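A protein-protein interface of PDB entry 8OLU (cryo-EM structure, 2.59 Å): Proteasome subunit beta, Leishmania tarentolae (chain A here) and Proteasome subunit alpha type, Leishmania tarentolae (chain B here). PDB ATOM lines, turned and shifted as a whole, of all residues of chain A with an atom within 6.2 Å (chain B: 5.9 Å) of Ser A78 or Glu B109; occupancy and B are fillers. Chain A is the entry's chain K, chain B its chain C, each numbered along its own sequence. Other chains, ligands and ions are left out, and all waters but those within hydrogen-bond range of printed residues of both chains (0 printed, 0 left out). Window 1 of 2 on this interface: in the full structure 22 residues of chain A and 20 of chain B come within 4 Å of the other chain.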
ATOM      1  N   GLN A  43       7.896  -6.549  23.404  1.00  0.00           N
ATOM      2  CA  GLN A  43       7.785  -5.911  24.683  1.00  0.00           C
ATOM      3  C   GLN A  43       9.173  -5.667  25.187  1.00  0.00           C
ATOM      4  O   GLN A  43       9.952  -6.591  25.150  1.00  0.00           O
ATOM      5  CB  GLN A  43       7.079  -6.789  25.711  1.00  0.00           C
ATOM      6  CG  GLN A  43       5.597  -6.833  25.464  1.00  0.00           C
ATOM      7  CD  GLN A  43       4.900  -7.822  26.353  1.00  0.00           C
ATOM      8  OE1 GLN A  43       5.483  -8.455  27.234  1.00  0.00           O
ATOM      9  NE2 GLN A  43       3.602  -7.932  26.130  1.00  0.00           N
ATOM     10  N   GLN A  72       1.034 -21.879  28.117  1.00  0.00           N
ATOM     11  CA  GLN A  72      -0.008 -21.240  27.361  1.00  0.00           C
ATOM     12  C   GLN A  72       0.352 -21.355  25.878  1.00  0.00           C
ATOM     13  O   GLN A  72       0.041 -20.473  25.078  1.00  0.00           O
ATOM     14  CB  GLN A  72      -0.167 -19.757  27.763  1.00  0.00           C
ATOM     15  CG  GLN A  72      -0.571 -19.477  29.243  1.00  0.00           C
ATOM     16  CD  GLN A  72      -0.707 -18.026  29.702  1.00  0.00           C
ATOM     17  OE1 GLN A  72      -0.872 -17.105  28.898  1.00  0.00           O
ATOM     18  NE2 GLN A  72      -0.656 -17.811  31.019  1.00  0.00           N
ATOM     19  N   HIS A  76       1.472 -14.937  23.151  1.00  0.00           N
ATOM     20  CA  HIS A  76       2.095 -13.781  23.754  1.00  0.00           C
ATOM     21  C   HIS A  76       1.074 -13.109  24.636  1.00  0.00           C
ATOM     22  O   HIS A  76      -0.101 -13.034  24.308  1.00  0.00           O
ATOM     23  CB  HIS A  76       2.745 -12.949  22.650  1.00  0.00           C
ATOM     24  CG  HIS A  76       3.808 -13.835  22.032  1.00  0.00           C
ATOM     25  ND1 HIS A  76       5.064 -14.042  22.596  1.00  0.00           N
ATOM     26  CD2 HIS A  76       3.701 -14.765  21.025  1.00  0.00           C
ATOM     27  CE1 HIS A  76       5.737 -14.952  21.894  1.00  0.00           C
ATOM     28  NE2 HIS A  76       4.903 -15.415  20.915  1.00  0.00           N
ATOM     29  N   SER A  77       1.524 -12.765  25.836  1.00  0.00           N
ATOM     30  CA  SER A  77       0.754 -11.923  26.726  1.00  0.00           C
ATOM     31  C   SER A  77       0.632 -10.544  26.085  1.00  0.00           C
ATOM     32  O   SER A  77       1.514 -10.111  25.359  1.00  0.00           O
ATOM     33  CB  SER A  77       1.447 -11.917  28.082  1.00  0.00           C
ATOM     34  OG  SER A  77       1.099 -10.799  28.918  1.00  0.00           O
ATOM     35  N   SER A  78      -0.468  -9.856  26.370  1.00  0.00           N
ATOM     36  CA  SER A  78      -0.656  -8.460  26.017  1.00  0.00           C
ATOM     37  C   SER A  78       0.255  -7.541  26.830  1.00  0.00           C
ATOM     38  O   SER A  78       0.757  -7.890  27.877  1.00  0.00           O
ATOM     39  CB  SER A  78      -2.094  -8.073  26.220  1.00  0.00           C
ATOM     40  OG  SER A  78      -2.422  -7.836  27.581  1.00  0.00           O
ATOM     41  N   CYS A  79       0.487  -6.347  26.331  1.00  0.00           N
ATOM     42  CA  CYS A  79       1.325  -5.421  27.045  1.00  0.00           C
ATOM     43  C   CYS A  79       0.650  -5.006  28.328  1.00  0.00           C
ATOM     44  O   CYS A  79       1.312  -4.911  29.325  1.00  0.00           O
ATOM     45  CB  CYS A  79       1.629  -4.194  26.198  1.00  0.00           C
ATOM     46  SG  CYS A  79       2.455  -4.600  24.626  1.00  0.00           S
ATOM     47  N   GLU A  80      -0.648  -4.805  28.347  1.00  0.00           N
ATOM     48  CA  GLU A  80      -1.273  -4.394  29.585  1.00  0.00           C
ATOM     49  C   GLU A  80      -1.139  -5.523  30.619  1.00  0.00           C
ATOM     50  O   GLU A  80      -0.875  -5.313  31.800  1.00  0.00           O
ATOM     51  CB  GLU A  80      -2.678  -3.824  29.318  1.00  0.00           C
ATOM     52  CG  GLU A  80      -3.205  -2.940  30.469  1.00  0.00           C
ATOM     53  CD  GLU A  80      -4.123  -1.725  30.192  1.00  0.00           C
ATOM     54  OE1 GLU A  80      -3.598  -0.588  29.959  1.00  0.00           O
ATOM     55  OE2 GLU A  80      -5.396  -1.880  30.243  1.00  0.00           O
ATOM     56  N   SER A  81      -1.288  -6.746  30.203  1.00  0.00           N
ATOM     57  CA  SER A  81      -1.048  -7.824  31.124  1.00  0.00           C
ATOM     58  C   SER A  81       0.313  -7.680  31.752  1.00  0.00           C
ATOM     59  O   SER A  81       0.476  -7.771  32.962  1.00  0.00           O
ATOM     60  CB  SER A  81      -1.098  -9.118  30.422  1.00  0.00           C
ATOM     61  OG  SER A  81      -1.181 -10.222  31.309  1.00  0.00           O
ATOM     62  N   THR A  82       1.311  -7.521  30.895  1.00  0.00           N
ATOM     63  CA  THR A  82       2.662  -7.586  31.376  1.00  0.00           C
ATOM     64  C   THR A  82       2.906  -6.424  32.305  1.00  0.00           C
ATOM     65  O   THR A  82       3.578  -6.532  33.300  1.00  0.00           O
ATOM     66  CB  THR A  82       3.662  -7.572  30.240  1.00  0.00           C
ATOM     67  OG1 THR A  82       3.504  -8.679  29.354  1.00  0.00           O
ATOM     68  CG2 THR A  82       5.078  -7.620  30.793  1.00  0.00           C
ATOM     69  N   ALA A  83       2.389  -5.286  31.965  1.00  0.00           N
ATOM     70  CA  ALA A  83       2.611  -4.131  32.783  1.00  0.00           C
ATOM     71  C   ALA A  83       1.970  -4.265  34.144  1.00  0.00           C
ATOM     72  O   ALA A  83       2.494  -3.785  35.116  1.00  0.00           O
ATOM     73  CB  ALA A  83       2.018  -2.953  32.077  1.00  0.00           C
ATOM     74  N   PHE A 107       7.852   0.743  30.319  1.00  0.00           N
ATOM     75  CA  PHE A 107       7.515  -0.502  29.699  1.00  0.00           C
ATOM     76  C   PHE A 107       6.842  -0.123  28.406  1.00  0.00           C
ATOM     77  O   PHE A 107       6.044   0.775  28.384  1.00  0.00           O
ATOM     78  CB  PHE A 107       6.726  -1.322  30.688  1.00  0.00           C
ATOM     79  CG  PHE A 107       6.106  -2.454  30.010  1.00  0.00           C
ATOM     80  CD1 PHE A 107       6.871  -3.447  29.481  1.00  0.00           C
ATOM     81  CD2 PHE A 107       4.807  -2.408  29.669  1.00  0.00           C
ATOM     82  CE1 PHE A 107       6.319  -4.491  28.752  1.00  0.00           C
ATOM     83  CE2 PHE A 107       4.263  -3.429  28.888  1.00  0.00           C
ATOM     84  CZ  PHE A 107       5.019  -4.478  28.426  1.00  0.00           C
ATOM     85  N   ASP A 111       1.145  -4.175  20.623  1.00  0.00           N
ATOM     86  CA  ASP A 111       0.203  -5.258  20.759  1.00  0.00           C
ATOM     87  C   ASP A 111      -0.285  -5.602  19.379  1.00  0.00           C
ATOM     88  O   ASP A 111      -0.778  -4.738  18.678  1.00  0.00           O
ATOM     89  CB  ASP A 111      -0.960  -4.883  21.677  1.00  0.00           C
ATOM     90  CG  ASP A 111      -0.780  -5.216  23.170  1.00  0.00           C
ATOM     91  OD1 ASP A 111      -0.295  -6.338  23.484  1.00  0.00           O
ATOM     92  OD2 ASP A 111      -1.161  -4.358  24.035  1.00  0.00           O
ATOM     93  N   ALA B 100      -9.984 -17.539  38.717  1.00  0.00           N
ATOM     94  CA  ALA B 100     -10.141 -16.607  37.661  1.00  0.00           C
ATOM     95  C   ALA B 100      -9.981 -15.173  38.157  1.00  0.00           C
ATOM     96  O   ALA B 100      -9.540 -14.306  37.429  1.00  0.00           O
ATOM     97  CB  ALA B 100     -11.499 -16.822  37.047  1.00  0.00           C
ATOM     98  N   HIS B 103      -6.317 -14.358  38.779  1.00  0.00           N
ATOM     99  CA  HIS B 103      -5.649 -14.046  37.542  1.00  0.00           C
ATOM    100  C   HIS B 103      -5.954 -12.610  37.160  1.00  0.00           C
ATOM    101  O   HIS B 103      -5.099 -11.821  36.809  1.00  0.00           O
ATOM    102  CB  HIS B 103      -6.093 -15.005  36.464  1.00  0.00           C
ATOM    103  CG  HIS B 103      -5.281 -14.853  35.233  1.00  0.00           C
ATOM    104  ND1 HIS B 103      -5.614 -14.011  34.218  1.00  0.00           N
ATOM    105  CD2 HIS B 103      -4.027 -15.340  35.013  1.00  0.00           C
ATOM    106  CE1 HIS B 103      -4.619 -14.029  33.342  1.00  0.00           C
ATOM    107  NE2 HIS B 103      -3.624 -14.856  33.805  1.00  0.00           N
ATOM    108  N   GLN B 104      -7.193 -12.223  37.281  1.00  0.00           N
ATOM    109  CA  GLN B 104      -7.503 -10.869  36.911  1.00  0.00           C
ATOM    110  C   GLN B 104      -6.884  -9.867  37.862  1.00  0.00           C
ATOM    111  O   GLN B 104      -6.603  -8.750  37.490  1.00  0.00           O
ATOM    112  CB  GLN B 104      -8.992 -10.696  36.851  1.00  0.00           C
ATOM    113  CG  GLN B 104      -9.394  -9.293  36.481  1.00  0.00           C
ATOM    114  CD  GLN B 104     -10.854  -9.441  36.199  1.00  0.00           C
ATOM    115  OE1 GLN B 104     -11.669  -9.280  37.123  1.00  0.00           O
ATOM    116  NE2 GLN B 104     -11.134  -9.913  34.972  1.00  0.00           N
ATOM    117  N   PHE B 107      -3.027  -9.867  36.503  1.00  0.00           N
ATOM    118  CA  PHE B 107      -2.791  -9.325  35.196  1.00  0.00           C
ATOM    119  C   PHE B 107      -3.796  -8.302  34.730  1.00  0.00           C
ATOM    120  O   PHE B 107      -3.623  -7.668  33.716  1.00  0.00           O
ATOM    121  CB  PHE B 107      -2.852 -10.464  34.221  1.00  0.00           C
ATOM    122  CG  PHE B 107      -1.780 -11.476  34.518  1.00  0.00           C
ATOM    123  CD1 PHE B 107      -0.486 -11.294  34.054  1.00  0.00           C
ATOM    124  CD2 PHE B 107      -2.034 -12.529  35.380  1.00  0.00           C
ATOM    125  CE1 PHE B 107       0.504 -12.195  34.391  1.00  0.00           C
ATOM    126  CE2 PHE B 107      -1.025 -13.397  35.778  1.00  0.00           C
ATOM    127  CZ  PHE B 107       0.241 -13.225  35.276  1.00  0.00           C
ATOM    128  N   GLN B 108      -4.913  -8.119  35.393  1.00  0.00           N
ATOM    129  CA  GLN B 108      -5.927  -7.227  34.873  1.00  0.00           C
ATOM    130  C   GLN B 108      -6.327  -7.588  33.476  1.00  0.00           C
ATOM    131  O   GLN B 108      -6.628  -6.734  32.700  1.00  0.00           O
ATOM    132  CB  GLN B 108      -5.469  -5.777  34.896  1.00  0.00           C
ATOM    133  CG  GLN B 108      -5.056  -5.315  36.311  1.00  0.00           C
ATOM    134  CD  GLN B 108      -6.241  -5.314  37.249  1.00  0.00           C
ATOM    135  OE1 GLN B 108      -7.318  -4.868  36.858  1.00  0.00           O
ATOM    136  NE2 GLN B 108      -6.055  -5.826  38.466  1.00  0.00           N
ATOM    137  N   GLU B 109      -6.459  -8.845  33.182  1.00  0.00           N
ATOM    138  CA  GLU B 109      -7.146  -9.224  31.965  1.00  0.00           C
ATOM    139  C   GLU B 109      -7.863 -10.521  32.273  1.00  0.00           C
ATOM    140  O   GLU B 109      -7.472 -11.219  33.186  1.00  0.00           O
ATOM    141  CB  GLU B 109      -6.178  -9.410  30.789  1.00  0.00           C
ATOM    142  CG  GLU B 109      -5.122 -10.471  31.055  1.00  0.00           C
ATOM    143  CD  GLU B 109      -4.470 -11.163  29.855  1.00  0.00           C
ATOM    144  OE1 GLU B 109      -3.826 -12.231  30.096  1.00  0.00           O
ATOM    145  OE2 GLU B 109      -4.564 -10.640  28.691  1.00  0.00           O
ATOM    146  N   PRO B 110      -8.860 -10.938  31.497  1.00  0.00           N
ATOM    147  CA  PRO B 110      -9.500 -12.225  31.731  1.00  0.00           C
ATOM    148  C   PRO B 110      -8.531 -13.385  31.626  1.00  0.00           C
ATOM    149  O   PRO B 110      -7.657 -13.392  30.791  1.00  0.00           O
ATOM    150  CB  PRO B 110     -10.467 -12.308  30.578  1.00  0.00           C
ATOM    151  CG  PRO B 110     -10.763 -10.876  30.316  1.00  0.00           C
ATOM    152  CD  PRO B 110      -9.381 -10.258  30.314  1.00  0.00           C
ATOM    153  N   MET B 111      -8.681 -14.326  32.527  1.00  0.00           N
ATOM    154  CA  MET B 111      -7.962 -15.581  32.474  1.00  0.00           C
ATOM    155  C   MET B 111      -8.406 -16.337  31.245  1.00  0.00           C
ATOM    156  O   MET B 111      -9.574 -16.274  30.878  1.00  0.00           O
ATOM    157  CB  MET B 111      -8.371 -16.427  33.669  1.00  0.00           C
ATOM    158  CG  MET B 111      -7.476 -17.565  33.852  1.00  0.00           C
ATOM    159  SD  MET B 111      -7.741 -18.388  35.376  1.00  0.00           S
ATOM    160  CE  MET B 111      -6.065 -18.915  35.715  1.00  0.00           C
ATOM    161  N   ARG B 147      -9.374 -14.312  24.003  1.00  0.00           N
ATOM    162  CA  ARG B 147      -8.901 -13.768  22.732  1.00  0.00           C
ATOM    163  C   ARG B 147      -7.930 -14.742  22.044  1.00  0.00           C
ATOM    164  O   ARG B 147      -7.644 -14.586  20.877  1.00  0.00           O
ATOM    165  CB  ARG B 147      -8.301 -12.401  23.033  1.00  0.00           C
ATOM    166  CG  ARG B 147      -6.981 -12.523  23.782  1.00  0.00           C
ATOM    167  CD  ARG B 147      -6.877 -11.372  24.781  1.00  0.00           C
ATOM    168  NE  ARG B 147      -5.486 -10.997  24.957  1.00  0.00           N
ATOM    169  CZ  ARG B 147      -4.844 -10.244  24.082  1.00  0.00           C
ATOM    170  NH1 ARG B 147      -5.522  -9.281  23.458  1.00  0.00           N
ATOM    171  NH2 ARG B 147      -3.564 -10.501  23.832  1.00  0.00           N
ATOM    172  N   TYR B 148      -7.473 -15.772  22.737  1.00  0.00           N
ATOM    173  CA  TYR B 148      -6.455 -16.658  22.219  1.00  0.00           C
ATOM    174  C   TYR B 148      -7.073 -17.699  21.299  1.00  0.00           C
ATOM    175  O   TYR B 148      -6.510 -18.040  20.266  1.00  0.00           O
ATOM    176  CB  TYR B 148      -5.696 -17.363  23.343  1.00  0.00           C
ATOM    177  CG  TYR B 148      -4.996 -16.430  24.296  1.00  0.00           C
ATOM    178  CD1 TYR B 148      -3.835 -15.759  23.921  1.00  0.00           C
ATOM    179  CD2 TYR B 148      -5.497 -16.186  25.575  1.00  0.00           C
ATOM    180  CE1 TYR B 148      -3.177 -14.904  24.799  1.00  0.00           C
ATOM    181  CE2 TYR B 148      -4.848 -15.337  26.461  1.00  0.00           C
ATOM    182  CZ  TYR B 148      -3.686 -14.693  26.070  1.00  0.00           C
ATOM    183  OH  TYR B 148      -3.036 -13.839  26.929  1.00  0.00           O
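Ser A78 touches just these residues of chain B: Glu B109 and Arg B147. Of chain A, only Ser A78 and Ser A81 come within 4 Å of Glu B109. Printed residues of chain A within 4 Å of Arg B147: Ser A78. Of the printed residues of chain B, Ser A81 touches Phe B107 and Glu B109. Of the printed residues of chain A, Tyr B148 touches His A76. The nearest residue of chain B that does not touch Ser A78 is Tyr B148 (4.8 Å). The nearest residue of chain A that does not touch Glu B109 is Ser A77 (5.3 Å).
Tyr B148 touches His A76. OE2 of Glu B109 touches OG of Ser A78 (3.7 Å). Ser A78 touches Arg B147 (CB to NH2, 3.7 Å). Phe B107 touches Ser A81. OG of Ser A81 touches OE1 of Glu B109 (3.5 Å).
The side-chain carboxylate (OE2) of Glu B109 is in salt-bridge range of the guanidinium group (NE) of Arg B147, at 3.9 Å. O of Ser A78 lies within hydrogen-bond range of OG1 of Thr A82, at 3.2 Å. OG of Ser A77 lies close to OG of Ser A81, 3.4 Å away. OG of Ser A78 is in hydrogen-bond range of N of Ser A81 (3.1 Å). The side-chain amide nitrogen (NE2) of Gln A43 sits at hydrogen-bond distance from the backbone carbonyl oxygen (O) of Ser A78 (3.3 Å).
Among the printed residues, no Asp or Glu carboxylate lies within 4 Å of a Lys or Arg side-chain nitrogen of the other chain.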
